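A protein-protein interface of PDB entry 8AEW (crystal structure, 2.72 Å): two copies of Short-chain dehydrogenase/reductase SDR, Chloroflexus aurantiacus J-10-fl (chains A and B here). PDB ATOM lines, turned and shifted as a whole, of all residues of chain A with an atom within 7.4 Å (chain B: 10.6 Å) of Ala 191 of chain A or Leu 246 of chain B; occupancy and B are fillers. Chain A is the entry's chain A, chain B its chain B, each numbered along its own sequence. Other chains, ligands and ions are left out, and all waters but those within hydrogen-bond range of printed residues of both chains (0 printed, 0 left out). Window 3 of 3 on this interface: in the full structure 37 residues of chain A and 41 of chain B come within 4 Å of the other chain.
The backbone carbonyl oxygen of Ser 272 of chain A lies within hydrogen-bond range of the guanidinium group of Arg 236 of chain B. N of Cys 238 of chain B lies within hydrogen-bond range of O of Gly 190 of chain A, at 3.1 Å. The side-chain carboxylate (OE2) of Glu 283 of chain B lies within salt-bridge range of the guanidinium group (NH2) of Arg 187 of chain A (3.1 Å). O of Gly 190 of chain A sits close to O of Arg 236 of chain B.
The backbone carbonyl oxygen (O) of Thr 234 of chain B is in hydrogen-bond range of the backbone NH (N) of Glu 283 of chain B (3.1 Å). O of His 280 of chain B sits at hydrogen-bond distance from N of Arg 236 of chain B, 3.3 Å away. The backbone carbonyl oxygen (O) of Gly 281 of chain B sits at hydrogen-bond distance from the backbone NH (N) of Arg 236 of chain B, 3.1 Å away. The backbone NH (N) of Leu 237 of chain B lies within hydrogen-bond range of the backbone carbonyl oxygen (O) of His 280 of chain B (3.1 Å). N of Gly 150 of chain A is in hydrogen-bond range of O of Gly 193 of chain A (2.9 Å).
Val 149 of chain A touches Leu 246 of chain B (CG1 to CD2, 3.6 Å). CG of Arg 187 of chain A touches CD of Arg 236 of chain B (3.6 Å). Leu 237 of chain B touches Gly 190 of chain A (CA to O, 3.8 Å). Ala 191 of chain A touches Arg 236 of chain B (N to O, 3.5 Å). Ala 191 of chain A touches Leu 246 of chain B. Arg 192 of chain A touches Leu 246 of chain B. Cys 238 of chain B touches Gly 193 of chain A (O to CA, 3.7 Å). Leu 237 of chain B touches Ser 272 of chain A (CB to CB, 3.9 Å). CA of Gly 281 of chain B touches O of Ser 272 of chain A, 3.1 Å away.
Of the printed residues of chain B, Ala 191 of chain A touches Arg 236 and Leu 246. Of the printed residues of chain A, Leu 246 of chain B touches Val 149 (3.6 Å), Ala 191 (3.3 Å) and Arg 192 (3.7 Å). Gly 190 of chain A touches three residues of chain B. Of the printed residues of chain B, Val 149 of chain A touches Leu 246. Of the printed residues of chain A, Arg 236 of chain B touches Arg 187, Gly 190, Ala 191 and Ser 272.
Of the 21 printed residues of chain B, 6 touch a printed residue of chain A. Hydrophobic or aromatic side chains of chain B that line the printed part of chain A: Leu 237 and Leu 246. Of the 13 printed residues of chain A, 7 touch a printed residue of chain B. Hydrophobic or aromatic side chains of chain A within 4 Å of the printed part of chain B: Val 149. Among the printed residues, 13 pairs touch across the chains. Among the printed residues, Asp or Glu carboxylates within 4 Å of a Lys or Arg side-chain nitrogen of the other chain: Arg 187 of chain A with Glu 283 of chain B.
No position is printed for both chains. Of the 13 pairs that touch across the chains among the printed residues, none has its exchanged pair printed and touching as well.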
ATOM      1  N   VAL A 149       4.022  -5.918  -3.773  1.00  0.00           N
ATOM      2  CA  VAL A 149       5.318  -5.346  -4.098  1.00  0.00           C
ATOM      3  C   VAL A 149       6.365  -6.053  -3.256  1.00  0.00           C
ATOM      4  O   VAL A 149       6.279  -6.049  -2.023  1.00  0.00           O
ATOM      5  CB  VAL A 149       5.322  -3.836  -3.795  1.00  0.00           C
ATOM      6  CG1 VAL A 149       6.673  -3.209  -4.116  1.00  0.00           C
ATOM      7  CG2 VAL A 149       4.190  -3.132  -4.507  1.00  0.00           C
ATOM      8  N   GLY A 150       7.368  -6.631  -3.899  1.00  0.00           N
ATOM      9  CA  GLY A 150       8.400  -7.387  -3.220  1.00  0.00           C
ATOM     10  C   GLY A 150       8.319  -8.873  -3.447  1.00  0.00           C
ATOM     11  O   GLY A 150       9.240  -9.597  -3.050  1.00  0.00           O
ATOM     12  N   ALA A 185       8.191 -11.273 -18.924  1.00  0.00           N
ATOM     13  CA  ALA A 185       7.342 -11.076 -17.743  1.00  0.00           C
ATOM     14  C   ALA A 185       8.056 -10.264 -16.674  1.00  0.00           C
ATOM     15  O   ALA A 185       7.398  -9.596 -15.871  1.00  0.00           O
ATOM     16  CB  ALA A 185       6.887 -12.415 -17.159  1.00  0.00           C
ATOM     17  N   ALA A 186       9.391 -10.316 -16.641  1.00  0.00           N
ATOM     18  CA  ALA A 186      10.155  -9.458 -15.742  1.00  0.00           C
ATOM     19  C   ALA A 186       9.912  -7.977 -16.039  1.00  0.00           C
ATOM     20  O   ALA A 186       9.824  -7.167 -15.110  1.00  0.00           O
ATOM     21  CB  ALA A 186      11.644  -9.797 -15.826  1.00  0.00           C
ATOM     22  N   ARG A 187       9.812  -7.601 -17.325  1.00  0.00           N
ATOM     23  CA  ARG A 187       9.506  -6.215 -17.680  1.00  0.00           C
ATOM     24  C   ARG A 187       8.180  -5.758 -17.104  1.00  0.00           C
ATOM     25  O   ARG A 187       8.108  -4.701 -16.468  1.00  0.00           O
ATOM     26  CB  ARG A 187       9.439  -6.026 -19.188  1.00  0.00           C
ATOM     27  CG  ARG A 187      10.720  -5.872 -19.929  1.00  0.00           C
ATOM     28  CD  ARG A 187      10.346  -5.671 -21.372  1.00  0.00           C
ATOM     29  NE  ARG A 187      11.497  -5.631 -22.258  1.00  0.00           N
ATOM     30  CZ  ARG A 187      11.405  -5.677 -23.584  1.00  0.00           C
ATOM     31  NH1 ARG A 187      10.236  -5.844 -24.187  1.00  0.00           N
ATOM     32  NH2 ARG A 187      12.512  -5.563 -24.323  1.00  0.00           N
ATOM     33  N   GLU A 188       7.105  -6.515 -17.364  1.00  0.00           N
ATOM     34  CA  GLU A 188       5.761  -6.063 -17.000  1.00  0.00           C
ATOM     35  C   GLU A 188       5.472  -6.219 -15.504  1.00  0.00           C
ATOM     36  O   GLU A 188       4.758  -5.396 -14.917  1.00  0.00           O
ATOM     37  CB  GLU A 188       4.709  -6.839 -17.780  1.00  0.00           C
ATOM     38  CG  GLU A 188       4.919  -6.894 -19.249  1.00  0.00           C
ATOM     39  CD  GLU A 188       3.767  -7.579 -19.960  1.00  0.00           C
ATOM     40  OE1 GLU A 188       2.737  -7.855 -19.302  1.00  0.00           O
ATOM     41  OE2 GLU A 188       3.921  -7.888 -21.171  1.00  0.00           O
ATOM     42  N   LEU A 189       5.995  -7.276 -14.879  1.00  0.00           N
ATOM     43  CA  LEU A 189       5.806  -7.467 -13.448  1.00  0.00           C
ATOM     44  C   LEU A 189       6.800  -6.641 -12.642  1.00  0.00           C
ATOM     45  O   LEU A 189       6.468  -6.158 -11.552  1.00  0.00           O
ATOM     46  CB  LEU A 189       5.934  -8.954 -13.095  1.00  0.00           C
ATOM     47  CG  LEU A 189       4.878  -9.874 -13.716  1.00  0.00           C
ATOM     48  CD1 LEU A 189       5.169 -11.333 -13.410  1.00  0.00           C
ATOM     49  CD2 LEU A 189       3.480  -9.479 -13.274  1.00  0.00           C
ATOM     50  N   GLY A 190       8.016  -6.478 -13.174  1.00  0.00           N
ATOM     51  CA  GLY A 190       8.964  -5.547 -12.598  1.00  0.00           C
ATOM     52  C   GLY A 190       8.407  -4.145 -12.465  1.00  0.00           C
ATOM     53  O   GLY A 190       8.732  -3.431 -11.513  1.00  0.00           O
ATOM     54  N   ALA A 191       7.548  -3.730 -13.398  1.00  0.00           N
ATOM     55  CA  ALA A 191       6.935  -2.419 -13.250  1.00  0.00           C
ATOM     56  C   ALA A 191       5.920  -2.391 -12.122  1.00  0.00           C
ATOM     57  O   ALA A 191       5.446  -1.312 -11.759  1.00  0.00           O
ATOM     58  CB  ALA A 191       6.256  -2.001 -14.556  1.00  0.00           C
ATOM     59  N   ARG A 192       5.597  -3.550 -11.554  1.00  0.00           N
ATOM     60  CA  ARG A 192       4.738  -3.677 -10.388  1.00  0.00           C
ATOM     61  C   ARG A 192       5.494  -3.929  -9.094  1.00  0.00           C
ATOM     62  O   ARG A 192       4.864  -4.032  -8.042  1.00  0.00           O
ATOM     63  CB  ARG A 192       3.744  -4.811 -10.620  1.00  0.00           C
ATOM     64  CG  ARG A 192       2.717  -4.483 -11.662  1.00  0.00           C
ATOM     65  CD  ARG A 192       1.848  -5.672 -11.935  1.00  0.00           C
ATOM     66  NE  ARG A 192       0.823  -5.352 -12.917  1.00  0.00           N
ATOM     67  CZ  ARG A 192      -0.002  -6.244 -13.447  1.00  0.00           C
ATOM     68  NH1 ARG A 192       0.084  -7.528 -13.135  1.00  0.00           N
ATOM     69  NH2 ARG A 192      -0.925  -5.841 -14.318  1.00  0.00           N
ATOM     70  N   GLY A 193       6.813  -4.020  -9.132  1.00  0.00           N
ATOM     71  CA  GLY A 193       7.548  -4.401  -7.947  1.00  0.00           C
ATOM     72  C   GLY A 193       7.642  -5.891  -7.712  1.00  0.00           C
ATOM     73  O   GLY A 193       8.116  -6.306  -6.649  1.00  0.00           O
ATOM     74  N   ILE A 194       7.271  -6.711  -8.694  1.00  0.00           N
ATOM     75  CA  ILE A 194       7.299  -8.164  -8.569  1.00  0.00           C
ATOM     76  C   ILE A 194       8.440  -8.661  -9.437  1.00  0.00           C
ATOM     77  O   ILE A 194       8.452  -8.410 -10.648  1.00  0.00           O
ATOM     78  CB  ILE A 194       5.967  -8.797  -9.007  1.00  0.00           C
ATOM     79  CG1 ILE A 194       4.810  -8.260  -8.170  1.00  0.00           C
ATOM     80  CG2 ILE A 194       6.020 -10.310  -8.863  1.00  0.00           C
ATOM     81  CD1 ILE A 194       3.476  -8.556  -8.766  1.00  0.00           C
ATOM     82  N   SER A 272      16.138  -9.136 -11.033  1.00  0.00           N
ATOM     83  CA  SER A 272      15.015  -9.492 -11.898  1.00  0.00           C
ATOM     84  C   SER A 272      15.481  -9.729 -13.332  1.00  0.00           C
ATOM     85  O   SER A 272      15.979  -8.805 -13.983  1.00  0.00           O
ATOM     86  CB  SER A 272      13.958  -8.385 -11.884  1.00  0.00           C
ATOM     87  OG  SER A 272      12.818  -8.744 -12.653  1.00  0.00           O
ATOM     88  N   LEU B 232      18.846   4.511 -15.008  1.00  0.00           N
ATOM     89  CA  LEU B 232      17.619   4.160 -14.304  1.00  0.00           C
ATOM     90  C   LEU B 232      16.554   3.641 -15.259  1.00  0.00           C
ATOM     91  O   LEU B 232      15.817   2.702 -14.929  1.00  0.00           O
ATOM     92  CB  LEU B 232      17.076   5.355 -13.526  1.00  0.00           C
ATOM     93  CG  LEU B 232      17.825   5.791 -12.276  1.00  0.00           C
ATOM     94  CD1 LEU B 232      17.108   6.956 -11.634  1.00  0.00           C
ATOM     95  CD2 LEU B 232      17.907   4.631 -11.328  1.00  0.00           C
ATOM     96  N   ASN B 233      16.472   4.220 -16.458  1.00  0.00           N
ATOM     97  CA  ASN B 233      15.402   3.847 -17.371  1.00  0.00           C
ATOM     98  C   ASN B 233      15.621   2.485 -18.005  1.00  0.00           C
ATOM     99  O   ASN B 233      14.665   1.904 -18.528  1.00  0.00           O
ATOM    100  CB  ASN B 233      15.219   4.913 -18.445  1.00  0.00           C
ATOM    101  CG  ASN B 233      14.508   6.149 -17.914  1.00  0.00           C
ATOM    102  OD1 ASN B 233      13.549   6.044 -17.137  1.00  0.00           O
ATOM    103  ND2 ASN B 233      14.970   7.328 -18.336  1.00  0.00           N
ATOM    104  N   THR B 234      16.839   1.955 -17.969  1.00  0.00           N
ATOM    105  CA  THR B 234      17.012   0.577 -18.402  1.00  0.00           C
ATOM    106  C   THR B 234      16.543  -0.444 -17.369  1.00  0.00           C
ATOM    107  O   THR B 234      16.493  -1.634 -17.697  1.00  0.00           O
ATOM    108  CB  THR B 234      18.475   0.302 -18.771  1.00  0.00           C
ATOM    109  OG1 THR B 234      19.328   0.549 -17.645  1.00  0.00           O
ATOM    110  CG2 THR B 234      18.897   1.175 -19.954  1.00  0.00           C
ATOM    111  N   MET B 235      16.166  -0.016 -16.157  1.00  0.00           N
ATOM    112  CA  MET B 235      15.845  -0.938 -15.065  1.00  0.00           C
ATOM    113  C   MET B 235      14.424  -1.485 -15.173  1.00  0.00           C
ATOM    114  O   MET B 235      13.464  -0.714 -15.261  1.00  0.00           O
ATOM    115  CB  MET B 235      16.017  -0.236 -13.716  1.00  0.00           C
ATOM    116  CG  MET B 235      17.443  -0.060 -13.273  1.00  0.00           C
ATOM    117  SD  MET B 235      17.495   0.992 -11.827  1.00  0.00           S
ATOM    118  CE  MET B 235      19.243   0.921 -11.452  1.00  0.00           C
ATOM    119  N   ARG B 236      14.295  -2.820 -15.135  1.00  0.00           N
ATOM    120  CA  ARG B 236      12.980  -3.464 -15.196  1.00  0.00           C
ATOM    121  C   ARG B 236      12.263  -3.486 -13.853  1.00  0.00           C
ATOM    122  O   ARG B 236      11.031  -3.423 -13.823  1.00  0.00           O
ATOM    123  CB  ARG B 236      13.109  -4.891 -15.738  1.00  0.00           C
ATOM    124  CG  ARG B 236      13.311  -4.908 -17.230  1.00  0.00           C
ATOM    125  CD  ARG B 236      13.624  -6.266 -17.810  1.00  0.00           C
ATOM    126  NE  ARG B 236      14.940  -6.732 -17.394  1.00  0.00           N
ATOM    127  CZ  ARG B 236      15.508  -7.834 -17.853  1.00  0.00           C
ATOM    128  NH1 ARG B 236      14.943  -8.546 -18.815  1.00  0.00           N
ATOM    129  NH2 ARG B 236      16.682  -8.215 -17.355  1.00  0.00           N
ATOM    130  N   LEU B 237      13.018  -3.555 -12.752  1.00  0.00           N
ATOM    131  CA  LEU B 237      12.495  -3.743 -11.402  1.00  0.00           C
ATOM    132  C   LEU B 237      12.407  -2.421 -10.645  1.00  0.00           C
ATOM    133  O   LEU B 237      13.431  -1.763 -10.418  1.00  0.00           O
ATOM    134  CB  LEU B 237      13.385  -4.705 -10.619  1.00  0.00           C
ATOM    135  CG  LEU B 237      12.959  -4.874  -9.164  1.00  0.00           C
ATOM    136  CD1 LEU B 237      11.572  -5.461  -9.135  1.00  0.00           C
ATOM    137  CD2 LEU B 237      13.962  -5.750  -8.436  1.00  0.00           C
ATOM    138  N   CYS B 238      11.191  -2.063 -10.224  1.00  0.00           N
ATOM    139  CA  CYS B 238      10.925  -0.958  -9.306  1.00  0.00           C
ATOM    140  C   CYS B 238      10.949  -1.460  -7.868  1.00  0.00           C
ATOM    141  O   CYS B 238      10.853  -2.663  -7.612  1.00  0.00           O
ATOM    142  CB  CYS B 238       9.562  -0.320  -9.563  1.00  0.00           C
ATOM    143  SG  CYS B 238       9.353   0.393 -11.154  1.00  0.00           S
ATOM    144  N   ARG B 239      11.109  -0.523  -6.928  1.00  0.00           N
ATOM    145  CA  ARG B 239      11.088  -0.841  -5.508  1.00  0.00           C
ATOM    146  C   ARG B 239      10.236   0.185  -4.778  1.00  0.00           C
ATOM    147  O   ARG B 239       9.995   1.289  -5.268  1.00  0.00           O
ATOM    148  CB  ARG B 239      12.503  -0.944  -4.915  1.00  0.00           C
ATOM    149  CG  ARG B 239      13.202  -2.166  -5.460  1.00  0.00           C
ATOM    150  CD  ARG B 239      14.508  -2.520  -4.838  1.00  0.00           C
ATOM    151  NE  ARG B 239      14.364  -3.142  -3.535  1.00  0.00           N
ATOM    152  CZ  ARG B 239      15.389  -3.497  -2.774  1.00  0.00           C
ATOM    153  NH1 ARG B 239      16.638  -3.339  -3.188  1.00  0.00           N
ATOM    154  NH2 ARG B 239      15.160  -4.044  -1.579  1.00  0.00           N
ATOM    155  N   ALA B 240       9.750  -0.211  -3.605  1.00  0.00           N
ATOM    156  CA  ALA B 240       8.912   0.662  -2.800  1.00  0.00           C
ATOM    157  C   ALA B 240       9.748   1.695  -2.049  1.00  0.00           C
ATOM    158  O   ALA B 240      10.893   1.444  -1.658  1.00  0.00           O
ATOM    159  CB  ALA B 240       8.086  -0.163  -1.816  1.00  0.00           C
ATOM    160  N   ASN B 241       9.162   2.863  -1.850  1.00  0.00           N
ATOM    161  CA  ASN B 241       9.762   3.838  -0.965  1.00  0.00           C
ATOM    162  C   ASN B 241       9.110   3.674   0.400  1.00  0.00           C
ATOM    163  O   ASN B 241       8.353   2.727   0.632  1.00  0.00           O
ATOM    164  CB  ASN B 241       9.647   5.267  -1.530  1.00  0.00           C
ATOM    165  CG  ASN B 241       8.205   5.777  -1.615  1.00  0.00           C
ATOM    166  OD1 ASN B 241       7.268   5.110  -1.201  1.00  0.00           O
ATOM    167  ND2 ASN B 241       8.040   6.981  -2.134  1.00  0.00           N
ATOM    168  N   ASP B 242       9.380   4.611   1.308  1.00  0.00           N
ATOM    169  CA  ASP B 242       8.892   4.485   2.677  1.00  0.00           C
ATOM    170  C   ASP B 242       7.379   4.576   2.754  1.00  0.00           C
ATOM    171  O   ASP B 242       6.758   3.948   3.624  1.00  0.00           O
ATOM    172  CB  ASP B 242       9.537   5.562   3.537  1.00  0.00           C
ATOM    173  CG  ASP B 242      11.006   5.338   3.696  1.00  0.00           C
ATOM    174  OD1 ASP B 242      11.407   4.149   3.773  1.00  0.00           O
ATOM    175  OD2 ASP B 242      11.758   6.332   3.695  1.00  0.00           O
ATOM    176  N   GLN B 243       6.778   5.355   1.866  1.00  0.00           N
ATOM    177  CA  GLN B 243       5.342   5.571   1.807  1.00  0.00           C
ATOM    178  C   GLN B 243       4.605   4.523   0.970  1.00  0.00           C
ATOM    179  O   GLN B 243       3.391   4.641   0.800  1.00  0.00           O
ATOM    180  CB  GLN B 243       5.075   6.979   1.288  1.00  0.00           C
ATOM    181  CG  GLN B 243       5.595   8.077   2.241  1.00  0.00           C
ATOM    182  CD  GLN B 243       7.137   8.120   2.343  1.00  0.00           C
ATOM    183  OE1 GLN B 243       7.700   8.026   3.438  1.00  0.00           O
ATOM    184  NE2 GLN B 243       7.815   8.226   1.191  1.00  0.00           N
ATOM    185  N   GLY B 244       5.316   3.549   0.387  1.00  0.00           N
ATOM    186  CA  GLY B 244       4.719   2.460  -0.367  1.00  0.00           C
ATOM    187  C   GLY B 244       4.559   2.667  -1.858  1.00  0.00           C
ATOM    188  O   GLY B 244       3.953   1.811  -2.516  1.00  0.00           O
ATOM    189  N   ALA B 245       5.040   3.786  -2.406  1.00  0.00           N
ATOM    190  CA  ALA B 245       5.023   4.060  -3.840  1.00  0.00           C
ATOM    191  C   ALA B 245       6.243   3.464  -4.540  1.00  0.00           C
ATOM    192  O   ALA B 245       7.296   3.256  -3.930  1.00  0.00           O
ATOM    193  CB  ALA B 245       4.954   5.561  -4.106  1.00  0.00           C
ATOM    194  N   LEU B 246       6.085   3.180  -5.834  1.00  0.00           N
ATOM    195  CA  LEU B 246       7.139   2.574  -6.642  1.00  0.00           C
ATOM    196  C   LEU B 246       8.029   3.622  -7.305  1.00  0.00           C
ATOM    197  O   LEU B 246       7.591   4.719  -7.664  1.00  0.00           O
ATOM    198  CB  LEU B 246       6.556   1.655  -7.720  1.00  0.00           C
ATOM    199  CG  LEU B 246       5.909   0.316  -7.367  1.00  0.00           C
ATOM    200  CD1 LEU B 246       5.399  -0.295  -8.634  1.00  0.00           C
ATOM    201  CD2 LEU B 246       6.886  -0.638  -6.690  1.00  0.00           C
ATOM    202  N   GLU B 247       9.288   3.251  -7.502  1.00  0.00           N
ATOM    203  CA  GLU B 247      10.280   4.184  -7.989  1.00  0.00           C
ATOM    204  C   GLU B 247      11.443   3.376  -8.545  1.00  0.00           C
ATOM    205  O   GLU B 247      11.660   2.232  -8.147  1.00  0.00           O
ATOM    206  CB  GLU B 247      10.735   5.109  -6.860  1.00  0.00           C
ATOM    207  CG  GLU B 247      11.613   4.423  -5.822  1.00  0.00           C
ATOM    208  CD  GLU B 247      11.855   5.275  -4.576  1.00  0.00           C
ATOM    209  OE1 GLU B 247      11.187   6.328  -4.396  1.00  0.00           O
ATOM    210  OE2 GLU B 247      12.745   4.901  -3.781  1.00  0.00           O
ATOM    211  N   ARG B 248      12.165   3.955  -9.496  1.00  0.00           N
ATOM    212  CA  ARG B 248      13.387   3.341  -9.995  1.00  0.00           C
ATOM    213  C   ARG B 248      14.533   4.043  -9.282  1.00  0.00           C
ATOM    214  O   ARG B 248      14.656   5.265  -9.368  1.00  0.00           O
ATOM    215  CB  ARG B 248      13.514   3.446 -11.523  1.00  0.00           C
ATOM    216  CG  ARG B 248      12.414   2.713 -12.333  1.00  0.00           C
ATOM    217  CD  ARG B 248      12.697   2.577 -13.834  1.00  0.00           C
ATOM    218  NE  ARG B 248      11.723   1.671 -14.432  1.00  0.00           N
ATOM    219  CZ  ARG B 248      10.472   2.045 -14.640  1.00  0.00           C
ATOM    220  NH1 ARG B 248      10.061   3.254 -14.288  1.00  0.00           N
ATOM    221  NH2 ARG B 248       9.590   1.164 -15.113  1.00  0.00           N
ATOM    222  N   ARG B 249      15.297   3.295  -8.498  1.00  0.00           N
ATOM    223  CA  ARG B 249      16.424   3.847  -7.763  1.00  0.00           C
ATOM    224  C   ARG B 249      17.564   2.858  -7.879  1.00  0.00           C
ATOM    225  O   ARG B 249      17.397   1.762  -8.417  1.00  0.00           O
ATOM    226  CB  ARG B 249      16.075   4.129  -6.291  1.00  0.00           C
ATOM    227  CG  ARG B 249      15.565   2.932  -5.492  1.00  0.00           C
ATOM    228  CD  ARG B 249      15.427   3.260  -4.006  1.00  0.00           C
ATOM    229  NE  ARG B 249      14.671   2.233  -3.301  1.00  0.00           N
ATOM    230  CZ  ARG B 249      15.175   1.073  -2.906  1.00  0.00           C
ATOM    231  NH1 ARG B 249      16.444   0.751  -3.140  1.00  0.00           N
ATOM    232  NH2 ARG B 249      14.380   0.200  -2.289  1.00  0.00           N
ATOM    233  N   HIS B 280      18.879  -4.200 -10.373  1.00  0.00           N
ATOM    234  CA  HIS B 280      17.433  -4.009 -10.536  1.00  0.00           C
ATOM    235  C   HIS B 280      16.984  -4.431 -11.939  1.00  0.00           C
ATOM    236  O   HIS B 280      16.131  -3.790 -12.561  1.00  0.00           O
ATOM    237  CB  HIS B 280      17.003  -2.565 -10.232  1.00  0.00           C
ATOM    238  CG  HIS B 280      17.076  -2.194  -8.780  1.00  0.00           C
ATOM    239  ND1 HIS B 280      16.870  -0.906  -8.332  1.00  0.00           N
ATOM    240  CD2 HIS B 280      17.325  -2.943  -7.675  1.00  0.00           C
ATOM    241  CE1 HIS B 280      16.985  -0.879  -7.012  1.00  0.00           C
ATOM    242  NE2 HIS B 280      17.269  -2.099  -6.590  1.00  0.00           N
ATOM    243  N   GLY B 281      17.587  -5.499 -12.453  1.00  0.00           N
ATOM    244  CA  GLY B 281      17.246  -5.950 -13.786  1.00  0.00           C
ATOM    245  C   GLY B 281      17.537  -4.921 -14.859  1.00  0.00           C
ATOM    246  O   GLY B 281      16.685  -4.692 -15.729  1.00  0.00           O
ATOM    247  N   GLU B 283      18.641  -3.805 -18.219  1.00  0.00           N
ATOM    248  CA  GLU B 283      18.520  -4.548 -19.462  1.00  0.00           C
ATOM    249  C   GLU B 283      19.507  -3.978 -20.463  1.00  0.00           C
ATOM    250  O   GLU B 283      19.342  -2.851 -20.941  1.00  0.00           O
ATOM    251  CB  GLU B 283      17.093  -4.474 -19.983  1.00  0.00           C
ATOM    252  CG  GLU B 283      16.906  -5.155 -21.293  1.00  0.00           C
ATOM    253  CD  GLU B 283      15.454  -5.169 -21.683  1.00  0.00           C
ATOM    254  OE1 GLU B 283      14.607  -4.725 -20.858  1.00  0.00           O
ATOM    255  OE2 GLU B 283      15.170  -5.601 -22.821  1.00  0.00           O
